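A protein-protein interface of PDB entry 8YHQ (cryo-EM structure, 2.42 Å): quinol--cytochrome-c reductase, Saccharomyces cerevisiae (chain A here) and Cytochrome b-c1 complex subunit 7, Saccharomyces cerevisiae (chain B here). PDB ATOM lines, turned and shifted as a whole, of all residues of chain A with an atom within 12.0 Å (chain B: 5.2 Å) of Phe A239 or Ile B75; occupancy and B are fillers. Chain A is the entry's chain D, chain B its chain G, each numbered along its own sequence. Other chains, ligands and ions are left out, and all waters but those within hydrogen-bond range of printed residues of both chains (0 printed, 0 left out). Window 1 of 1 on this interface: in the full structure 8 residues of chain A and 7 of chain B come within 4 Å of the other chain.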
ATOM      1  N   TRP A 231      17.435   2.010  -4.300  1.00  0.00           N
ATOM      2  CA  TRP A 231      16.858   3.167  -4.973  1.00  0.00           C
ATOM      3  C   TRP A 231      15.709   2.796  -5.902  1.00  0.00           C
ATOM      4  O   TRP A 231      15.195   3.664  -6.614  1.00  0.00           O
ATOM      5  CB  TRP A 231      17.942   3.909  -5.761  1.00  0.00           C
ATOM      6  CG  TRP A 231      18.572   5.017  -5.024  1.00  0.00           C
ATOM      7  CD1 TRP A 231      19.520   4.920  -4.061  1.00  0.00           C
ATOM      8  CD2 TRP A 231      18.302   6.408  -5.183  1.00  0.00           C
ATOM      9  NE1 TRP A 231      19.860   6.154  -3.608  1.00  0.00           N
ATOM     10  CE2 TRP A 231      19.126   7.092  -4.281  1.00  0.00           C
ATOM     11  CE3 TRP A 231      17.444   7.143  -6.001  1.00  0.00           C
ATOM     12  CZ2 TRP A 231      19.118   8.471  -4.170  1.00  0.00           C
ATOM     13  CZ3 TRP A 231      17.438   8.507  -5.886  1.00  0.00           C
ATOM     14  CH2 TRP A 231      18.268   9.157  -4.981  1.00  0.00           C
ATOM     15  N   ALA A 232      15.279   1.537  -5.903  1.00  0.00           N
ATOM     16  CA  ALA A 232      14.327   1.078  -6.905  1.00  0.00           C
ATOM     17  C   ALA A 232      12.909   1.529  -6.593  1.00  0.00           C
ATOM     18  O   ALA A 232      12.095   1.680  -7.509  1.00  0.00           O
ATOM     19  CB  ALA A 232      14.403  -0.439  -7.021  1.00  0.00           C
ATOM     20  N   GLY A 233      12.592   1.751  -5.318  1.00  0.00           N
ATOM     21  CA  GLY A 233      11.300   2.306  -4.969  1.00  0.00           C
ATOM     22  C   GLY A 233      11.085   3.714  -5.483  1.00  0.00           C
ATOM     23  O   GLY A 233      10.001   4.037  -5.971  1.00  0.00           O
ATOM     24  N   ILE A 234      12.106   4.564  -5.385  1.00  0.00           N
ATOM     25  CA  ILE A 234      11.988   5.954  -5.802  1.00  0.00           C
ATOM     26  C   ILE A 234      11.922   6.084  -7.316  1.00  0.00           C
ATOM     27  O   ILE A 234      11.217   6.957  -7.831  1.00  0.00           O
ATOM     28  CB  ILE A 234      13.157   6.779  -5.229  1.00  0.00           C
ATOM     29  CG1 ILE A 234      13.270   6.651  -3.706  1.00  0.00           C
ATOM     30  CG2 ILE A 234      13.031   8.227  -5.620  1.00  0.00           C
ATOM     31  CD1 ILE A 234      12.146   7.196  -2.915  1.00  0.00           C
ATOM     32  N   LYS A 235      12.646   5.245  -8.054  1.00  0.00           N
ATOM     33  CA  LYS A 235      12.731   5.377  -9.503  1.00  0.00           C
ATOM     34  C   LYS A 235      11.455   4.968 -10.231  1.00  0.00           C
ATOM     35  O   LYS A 235      11.209   5.468 -11.332  1.00  0.00           O
ATOM     36  CB  LYS A 235      13.899   4.552 -10.042  1.00  0.00           C
ATOM     37  CG  LYS A 235      15.264   5.027  -9.609  1.00  0.00           C
ATOM     38  CD  LYS A 235      15.721   6.211 -10.412  1.00  0.00           C
ATOM     39  CE  LYS A 235      17.058   6.742  -9.932  1.00  0.00           C
ATOM     40  NZ  LYS A 235      18.177   6.329 -10.800  1.00  0.00           N
ATOM     41  N   THR A 236      10.643   4.084  -9.650  1.00  0.00           N
ATOM     42  CA  THR A 236       9.424   3.593 -10.286  1.00  0.00           C
ATOM     43  C   THR A 236       8.154   4.117  -9.620  1.00  0.00           C
ATOM     44  O   THR A 236       7.052   3.738 -10.027  1.00  0.00           O
ATOM     45  CB  THR A 236       9.417   2.063 -10.298  1.00  0.00           C
ATOM     46  OG1 THR A 236       9.518   1.563  -8.963  1.00  0.00           O
ATOM     47  CG2 THR A 236      10.572   1.528 -11.118  1.00  0.00           C
ATOM     48  N   ARG A 237       8.282   4.977  -8.617  1.00  0.00           N
ATOM     49  CA  ARG A 237       7.136   5.604  -7.977  1.00  0.00           C
ATOM     50  C   ARG A 237       6.353   6.458  -8.970  1.00  0.00           C
ATOM     51  O   ARG A 237       6.927   7.089  -9.859  1.00  0.00           O
ATOM     52  CB  ARG A 237       7.639   6.426  -6.788  1.00  0.00           C
ATOM     53  CG  ARG A 237       6.786   7.522  -6.249  1.00  0.00           C
ATOM     54  CD  ARG A 237       7.524   8.204  -5.120  1.00  0.00           C
ATOM     55  NE  ARG A 237       8.493   9.157  -5.645  1.00  0.00           N
ATOM     56  CZ  ARG A 237       9.137  10.071  -4.931  1.00  0.00           C
ATOM     57  NH1 ARG A 237       9.989  10.875  -5.533  1.00  0.00           N
ATOM     58  NH2 ARG A 237       8.944  10.196  -3.629  1.00  0.00           N
ATOM     59  N   LYS A 238       5.028   6.474  -8.804  1.00  0.00           N
ATOM     60  CA  LYS A 238       4.108   7.107  -9.737  1.00  0.00           C
ATOM     61  C   LYS A 238       3.194   8.101  -9.027  1.00  0.00           C
ATOM     62  O   LYS A 238       2.889   7.949  -7.843  1.00  0.00           O
ATOM     63  CB  LYS A 238       3.285   6.049 -10.449  1.00  0.00           C
ATOM     64  CG  LYS A 238       4.080   5.334 -11.501  1.00  0.00           C
ATOM     65  CD  LYS A 238       3.317   4.250 -12.166  1.00  0.00           C
ATOM     66  CE  LYS A 238       4.233   3.385 -12.994  1.00  0.00           C
ATOM     67  NZ  LYS A 238       5.114   4.131 -13.910  1.00  0.00           N
ATOM     68  N   PHE A 239       2.769   9.126  -9.772  1.00  0.00           N
ATOM     69  CA  PHE A 239       1.947  10.218  -9.264  1.00  0.00           C
ATOM     70  C   PHE A 239       0.718  10.423 -10.143  1.00  0.00           C
ATOM     71  O   PHE A 239       0.774  10.262 -11.364  1.00  0.00           O
ATOM     72  CB  PHE A 239       2.725  11.532  -9.204  1.00  0.00           C
ATOM     73  CG  PHE A 239       3.733  11.600  -8.097  1.00  0.00           C
ATOM     74  CD1 PHE A 239       3.356  11.972  -6.828  1.00  0.00           C
ATOM     75  CD2 PHE A 239       5.060  11.314  -8.329  1.00  0.00           C
ATOM     76  CE1 PHE A 239       4.274  12.044  -5.819  1.00  0.00           C
ATOM     77  CE2 PHE A 239       5.974  11.386  -7.315  1.00  0.00           C
ATOM     78  CZ  PHE A 239       5.581  11.751  -6.064  1.00  0.00           C
ATOM     79  N   VAL A 240      -0.391  10.790  -9.504  1.00  0.00           N
ATOM     80  CA  VAL A 240      -1.651  11.091 -10.181  1.00  0.00           C
ATOM     81  C   VAL A 240      -2.239  12.350  -9.552  1.00  0.00           C
ATOM     82  O   VAL A 240      -2.093  12.569  -8.347  1.00  0.00           O
ATOM     83  CB  VAL A 240      -2.642   9.908 -10.087  1.00  0.00           C
ATOM     84  CG1 VAL A 240      -4.004  10.305 -10.575  1.00  0.00           C
ATOM     85  CG2 VAL A 240      -2.148   8.733 -10.886  1.00  0.00           C
ATOM     86  N   PHE A 241      -2.894  13.178 -10.369  1.00  0.00           N
ATOM     87  CA  PHE A 241      -3.533  14.413  -9.918  1.00  0.00           C
ATOM     88  C   PHE A 241      -5.005  14.414 -10.306  1.00  0.00           C
ATOM     89  O   PHE A 241      -5.342  14.169 -11.467  1.00  0.00           O
ATOM     90  CB  PHE A 241      -2.842  15.636 -10.518  1.00  0.00           C
ATOM     91  CG  PHE A 241      -3.322  16.953  -9.969  1.00  0.00           C
ATOM     92  CD1 PHE A 241      -3.295  17.225  -8.618  1.00  0.00           C
ATOM     93  CD2 PHE A 241      -3.788  17.930 -10.819  1.00  0.00           C
ATOM     94  CE1 PHE A 241      -3.735  18.432  -8.137  1.00  0.00           C
ATOM     95  CE2 PHE A 241      -4.220  19.129 -10.340  1.00  0.00           C
ATOM     96  CZ  PHE A 241      -4.196  19.380  -9.000  1.00  0.00           C
ATOM     97  N   ASN A 242      -5.867  14.702  -9.337  1.00  0.00           N
ATOM     98  CA  ASN A 242      -7.297  14.914  -9.566  1.00  0.00           C
ATOM     99  C   ASN A 242      -7.652  16.309  -9.059  1.00  0.00           C
ATOM    100  O   ASN A 242      -7.609  16.532  -7.834  1.00  0.00           O
ATOM    101  CB  ASN A 242      -8.135  13.856  -8.849  1.00  0.00           C
ATOM    102  CG  ASN A 242      -7.757  12.450  -9.243  1.00  0.00           C
ATOM    103  OD1 ASN A 242      -7.164  11.706  -8.463  1.00  0.00           O
ATOM    104  ND2 ASN A 242      -8.106  12.074 -10.457  1.00  0.00           N
ATOM    105  N   PRO A 243      -7.996  17.280  -9.913  1.00  0.00           N
ATOM    106  CA  PRO A 243      -8.168  18.663  -9.437  1.00  0.00           C
ATOM    107  C   PRO A 243      -9.294  18.779  -8.424  1.00  0.00           C
ATOM    108  O   PRO A 243     -10.444  18.436  -8.733  1.00  0.00           O
ATOM    109  CB  PRO A 243      -8.503  19.442 -10.717  1.00  0.00           C
ATOM    110  CG  PRO A 243      -8.041  18.616 -11.799  1.00  0.00           C
ATOM    111  CD  PRO A 243      -8.197  17.211 -11.368  1.00  0.00           C
ATOM    112  N   ALA B  71       1.861  23.037  -7.837  1.00  0.00           N
ATOM    113  CA  ALA B  71       2.568  22.075  -6.999  1.00  0.00           C
ATOM    114  C   ALA B  71       2.721  20.726  -7.690  1.00  0.00           C
ATOM    115  O   ALA B  71       3.723  20.032  -7.492  1.00  0.00           O
ATOM    116  CB  ALA B  71       1.844  21.910  -5.667  1.00  0.00           C
ATOM    117  N   TYR B  72       1.739  20.329  -8.495  1.00  0.00           N
ATOM    118  CA  TYR B  72       1.801  19.032  -9.153  1.00  0.00           C
ATOM    119  C   TYR B  72       2.789  19.044 -10.313  1.00  0.00           C
ATOM    120  O   TYR B  72       3.519  18.072 -10.527  1.00  0.00           O
ATOM    121  CB  TYR B  72       0.414  18.618  -9.633  1.00  0.00           C
ATOM    122  CG  TYR B  72       0.429  17.410 -10.523  1.00  0.00           C
ATOM    123  CD1 TYR B  72       0.857  16.180 -10.052  1.00  0.00           C
ATOM    124  CD2 TYR B  72       0.031  17.498 -11.840  1.00  0.00           C
ATOM    125  CE1 TYR B  72       0.880  15.091 -10.857  1.00  0.00           C
ATOM    126  CE2 TYR B  72       0.049  16.409 -12.654  1.00  0.00           C
ATOM    127  CZ  TYR B  72       0.474  15.204 -12.161  1.00  0.00           C
ATOM    128  OH  TYR B  72       0.490  14.114 -12.985  1.00  0.00           O
ATOM    129  N   ARG B  73       2.812  20.132 -11.082  1.00  0.00           N
ATOM    130  CA  ARG B  73       3.757  20.245 -12.185  1.00  0.00           C
ATOM    131  C   ARG B  73       5.196  20.204 -11.689  1.00  0.00           C
ATOM    132  O   ARG B  73       6.083  19.695 -12.381  1.00  0.00           O
ATOM    133  CB  ARG B  73       3.498  21.531 -12.962  1.00  0.00           C
ATOM    134  CG  ARG B  73       2.236  21.515 -13.775  1.00  0.00           C
ATOM    135  CD  ARG B  73       2.164  22.671 -14.753  1.00  0.00           C
ATOM    136  NE  ARG B  73       2.205  23.964 -14.088  1.00  0.00           N
ATOM    137  CZ  ARG B  73       1.149  24.694 -13.738  1.00  0.00           C
ATOM    138  NH1 ARG B  73       1.349  25.847 -13.135  1.00  0.00           N
ATOM    139  NH2 ARG B  73      -0.095  24.305 -13.982  1.00  0.00           N
ATOM    140  N   ILE B  74       5.445  20.726 -10.489  1.00  0.00           N
ATOM    141  CA  ILE B  74       6.799  20.792  -9.962  1.00  0.00           C
ATOM    142  C   ILE B  74       7.241  19.430  -9.441  1.00  0.00           C
ATOM    143  O   ILE B  74       8.403  19.041  -9.598  1.00  0.00           O
ATOM    144  CB  ILE B  74       6.881  21.902  -8.893  1.00  0.00           C
ATOM    145  CG1 ILE B  74       7.074  23.257  -9.583  1.00  0.00           C
ATOM    146  CG2 ILE B  74       7.991  21.660  -7.878  1.00  0.00           C
ATOM    147  CD1 ILE B  74       6.775  24.464  -8.736  1.00  0.00           C
ATOM    148  N   ILE B  75       6.331  18.687  -8.812  1.00  0.00           N
ATOM    149  CA  ILE B  75       6.641  17.341  -8.345  1.00  0.00           C
ATOM    150  C   ILE B  75       6.857  16.400  -9.524  1.00  0.00           C
ATOM    151  O   ILE B  75       7.783  15.583  -9.520  1.00  0.00           O
ATOM    152  CB  ILE B  75       5.526  16.858  -7.403  1.00  0.00           C
ATOM    153  CG1 ILE B  75       5.705  17.512  -6.036  1.00  0.00           C
ATOM    154  CG2 ILE B  75       5.498  15.344  -7.275  1.00  0.00           C
ATOM    155  CD1 ILE B  75       4.522  17.406  -5.124  1.00  0.00           C
ATOM    156  N   ARG B  76       6.001  16.489 -10.538  1.00  0.00           N
ATOM    157  CA  ARG B  76       6.138  15.657 -11.726  1.00  0.00           C
ATOM    158  C   ARG B  76       7.468  15.892 -12.442  1.00  0.00           C
ATOM    159  O   ARG B  76       8.039  14.961 -13.019  1.00  0.00           O
ATOM    160  CB  ARG B  76       4.953  15.918 -12.653  1.00  0.00           C
ATOM    161  CG  ARG B  76       4.905  15.103 -13.916  1.00  0.00           C
ATOM    162  CD  ARG B  76       3.651  15.375 -14.707  1.00  0.00           C
ATOM    163  NE  ARG B  76       3.596  16.723 -15.251  1.00  0.00           N
ATOM    164  CZ  ARG B  76       2.719  17.140 -16.155  1.00  0.00           C
ATOM    165  NH1 ARG B  76       2.760  18.388 -16.575  1.00  0.00           N
ATOM    166  NH2 ARG B  76       1.800  16.328 -16.647  1.00  0.00           N
ATOM    167  N   ALA B  77       7.977  17.125 -12.422  1.00  0.00           N
ATOM    168  CA  ALA B  77       9.219  17.430 -13.125  1.00  0.00           C
ATOM    169  C   ALA B  77      10.442  16.921 -12.369  1.00  0.00           C
ATOM    170  O   ALA B  77      11.418  16.491 -12.989  1.00  0.00           O
ATOM    171  CB  ALA B  77       9.332  18.930 -13.368  1.00  0.00           C
ATOM    172  N   HIS B  78      10.427  16.991 -11.038  1.00  0.00           N
ATOM    173  CA  HIS B  78      11.517  16.416 -10.259  1.00  0.00           C
ATOM    174  C   HIS B  78      11.627  14.912 -10.489  1.00  0.00           C
ATOM    175  O   HIS B  78      12.732  14.375 -10.606  1.00  0.00           O
ATOM    176  CB  HIS B  78      11.319  16.703  -8.772  1.00  0.00           C
ATOM    177  CG  HIS B  78      11.707  18.083  -8.348  1.00  0.00           C
ATOM    178  ND1 HIS B  78      12.852  18.709  -8.783  1.00  0.00           N
ATOM    179  CD2 HIS B  78      11.105  18.950  -7.505  1.00  0.00           C
ATOM    180  CE1 HIS B  78      12.933  19.906  -8.236  1.00  0.00           C
ATOM    181  NE2 HIS B  78      11.885  20.078  -7.457  1.00  0.00           N
ATOM    182  N   GLN B  79      10.491  14.217 -10.541  1.00  0.00           N
ATOM    183  CA  GLN B  79      10.497  12.774 -10.747  1.00  0.00           C
ATOM    184  C   GLN B  79      10.946  12.422 -12.157  1.00  0.00           C
ATOM    185  O   GLN B  79      11.619  11.410 -12.365  1.00  0.00           O
ATOM    186  CB  GLN B  79       9.102  12.210 -10.454  1.00  0.00           C
ATOM    187  CG  GLN B  79       8.950  10.704 -10.500  1.00  0.00           C
ATOM    188  CD  GLN B  79       9.597   9.998  -9.338  1.00  0.00           C
ATOM    189  OE1 GLN B  79       9.682  10.532  -8.236  1.00  0.00           O
ATOM    190  NE2 GLN B  79      10.055   8.786  -9.574  1.00  0.00           N
ATOM    191  N   THR B  80      10.575  13.242 -13.140  1.00  0.00           N
ATOM    192  CA  THR B  80      11.014  13.009 -14.508  1.00  0.00           C
ATOM    193  C   THR B  80      12.524  13.149 -14.658  1.00  0.00           C
ATOM    194  O   THR B  80      13.120  12.506 -15.527  1.00  0.00           O
ATOM    195  CB  THR B  80      10.293  13.972 -15.452  1.00  0.00           C
ATOM    196  OG1 THR B  80       8.884  13.898 -15.226  1.00  0.00           O
ATOM    197  CG2 THR B  80      10.560  13.638 -16.890  1.00  0.00           C
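The side-chain amide oxygen (OE1) of Gln B79 lies within hydrogen-bond range of the guanidinium group (NH1) of Arg A237 (2.7 Å). The side-chain amide nitrogen (NE2) of Gln B79 sits at hydrogen-bond distance from the backbone carbonyl oxygen (O) of Ile A234, at 2.8 Å.
Gln B79 touches Lys A235. Phe A239 touches Ile B75. OE1 of Gln B79 touches CE2 of Phe A239, 3.9 Å away. Tyr B72 touches Phe A241.
Of chain B, only Ile B75 and Gln B79 come within 4 Å of Phe A239. Of chain A, only Phe A239 (3.8 Å) comes within 4 Å of Ile B75. Ala B71 touches none of the printed residues of chain A. No residue of chain A comes within 4 Å of Ile B74. No residue of chain A comes within 4 Å of Ala B77. Gln B79 touches just these residues of chain A: Ile A234 (2.8 Å), Lys A235 (3.9 Å), Arg A237 (2.7 Å) and Phe A239 (3.9 Å). Printed residues of chain B within 4 Å of Ile A234: Gln B79 (2.8 Å). Of the printed residues of chain B, Arg A237 touches Gln B79 (2.7 Å). Printed residues of chain B within 4 Å of Lys A235: Gln B79 (3.9 Å). Printed residues of chain B within 4 Å of Phe A241: Tyr B72 (3.7 Å). Arg B76 touches none of the printed residues of chain A. Gly A233 touches none of the printed residues of chain B. The nearest printed residue of chain B that does not touch Phe A241 is Ala B71 (6.9 Å).
Hydrophobic or aromatic side chains of chain B that line the printed part of chain A: Tyr B72 and Ile B75. Printed residues of chain A that touch a printed residue of chain B: Ile A234, Lys A235, Arg A237, Phe A239 and Phe A241. Hydrophobic or aromatic side chains of chain A that line the printed part of chain B: Phe A239 and Phe A241. Among the printed residues, 6 pairs touch across the chains. Among the printed residues, no Asp or Glu carboxylate lies within 4 Å of a Lys or Arg side-chain nitrogen of the other chain.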
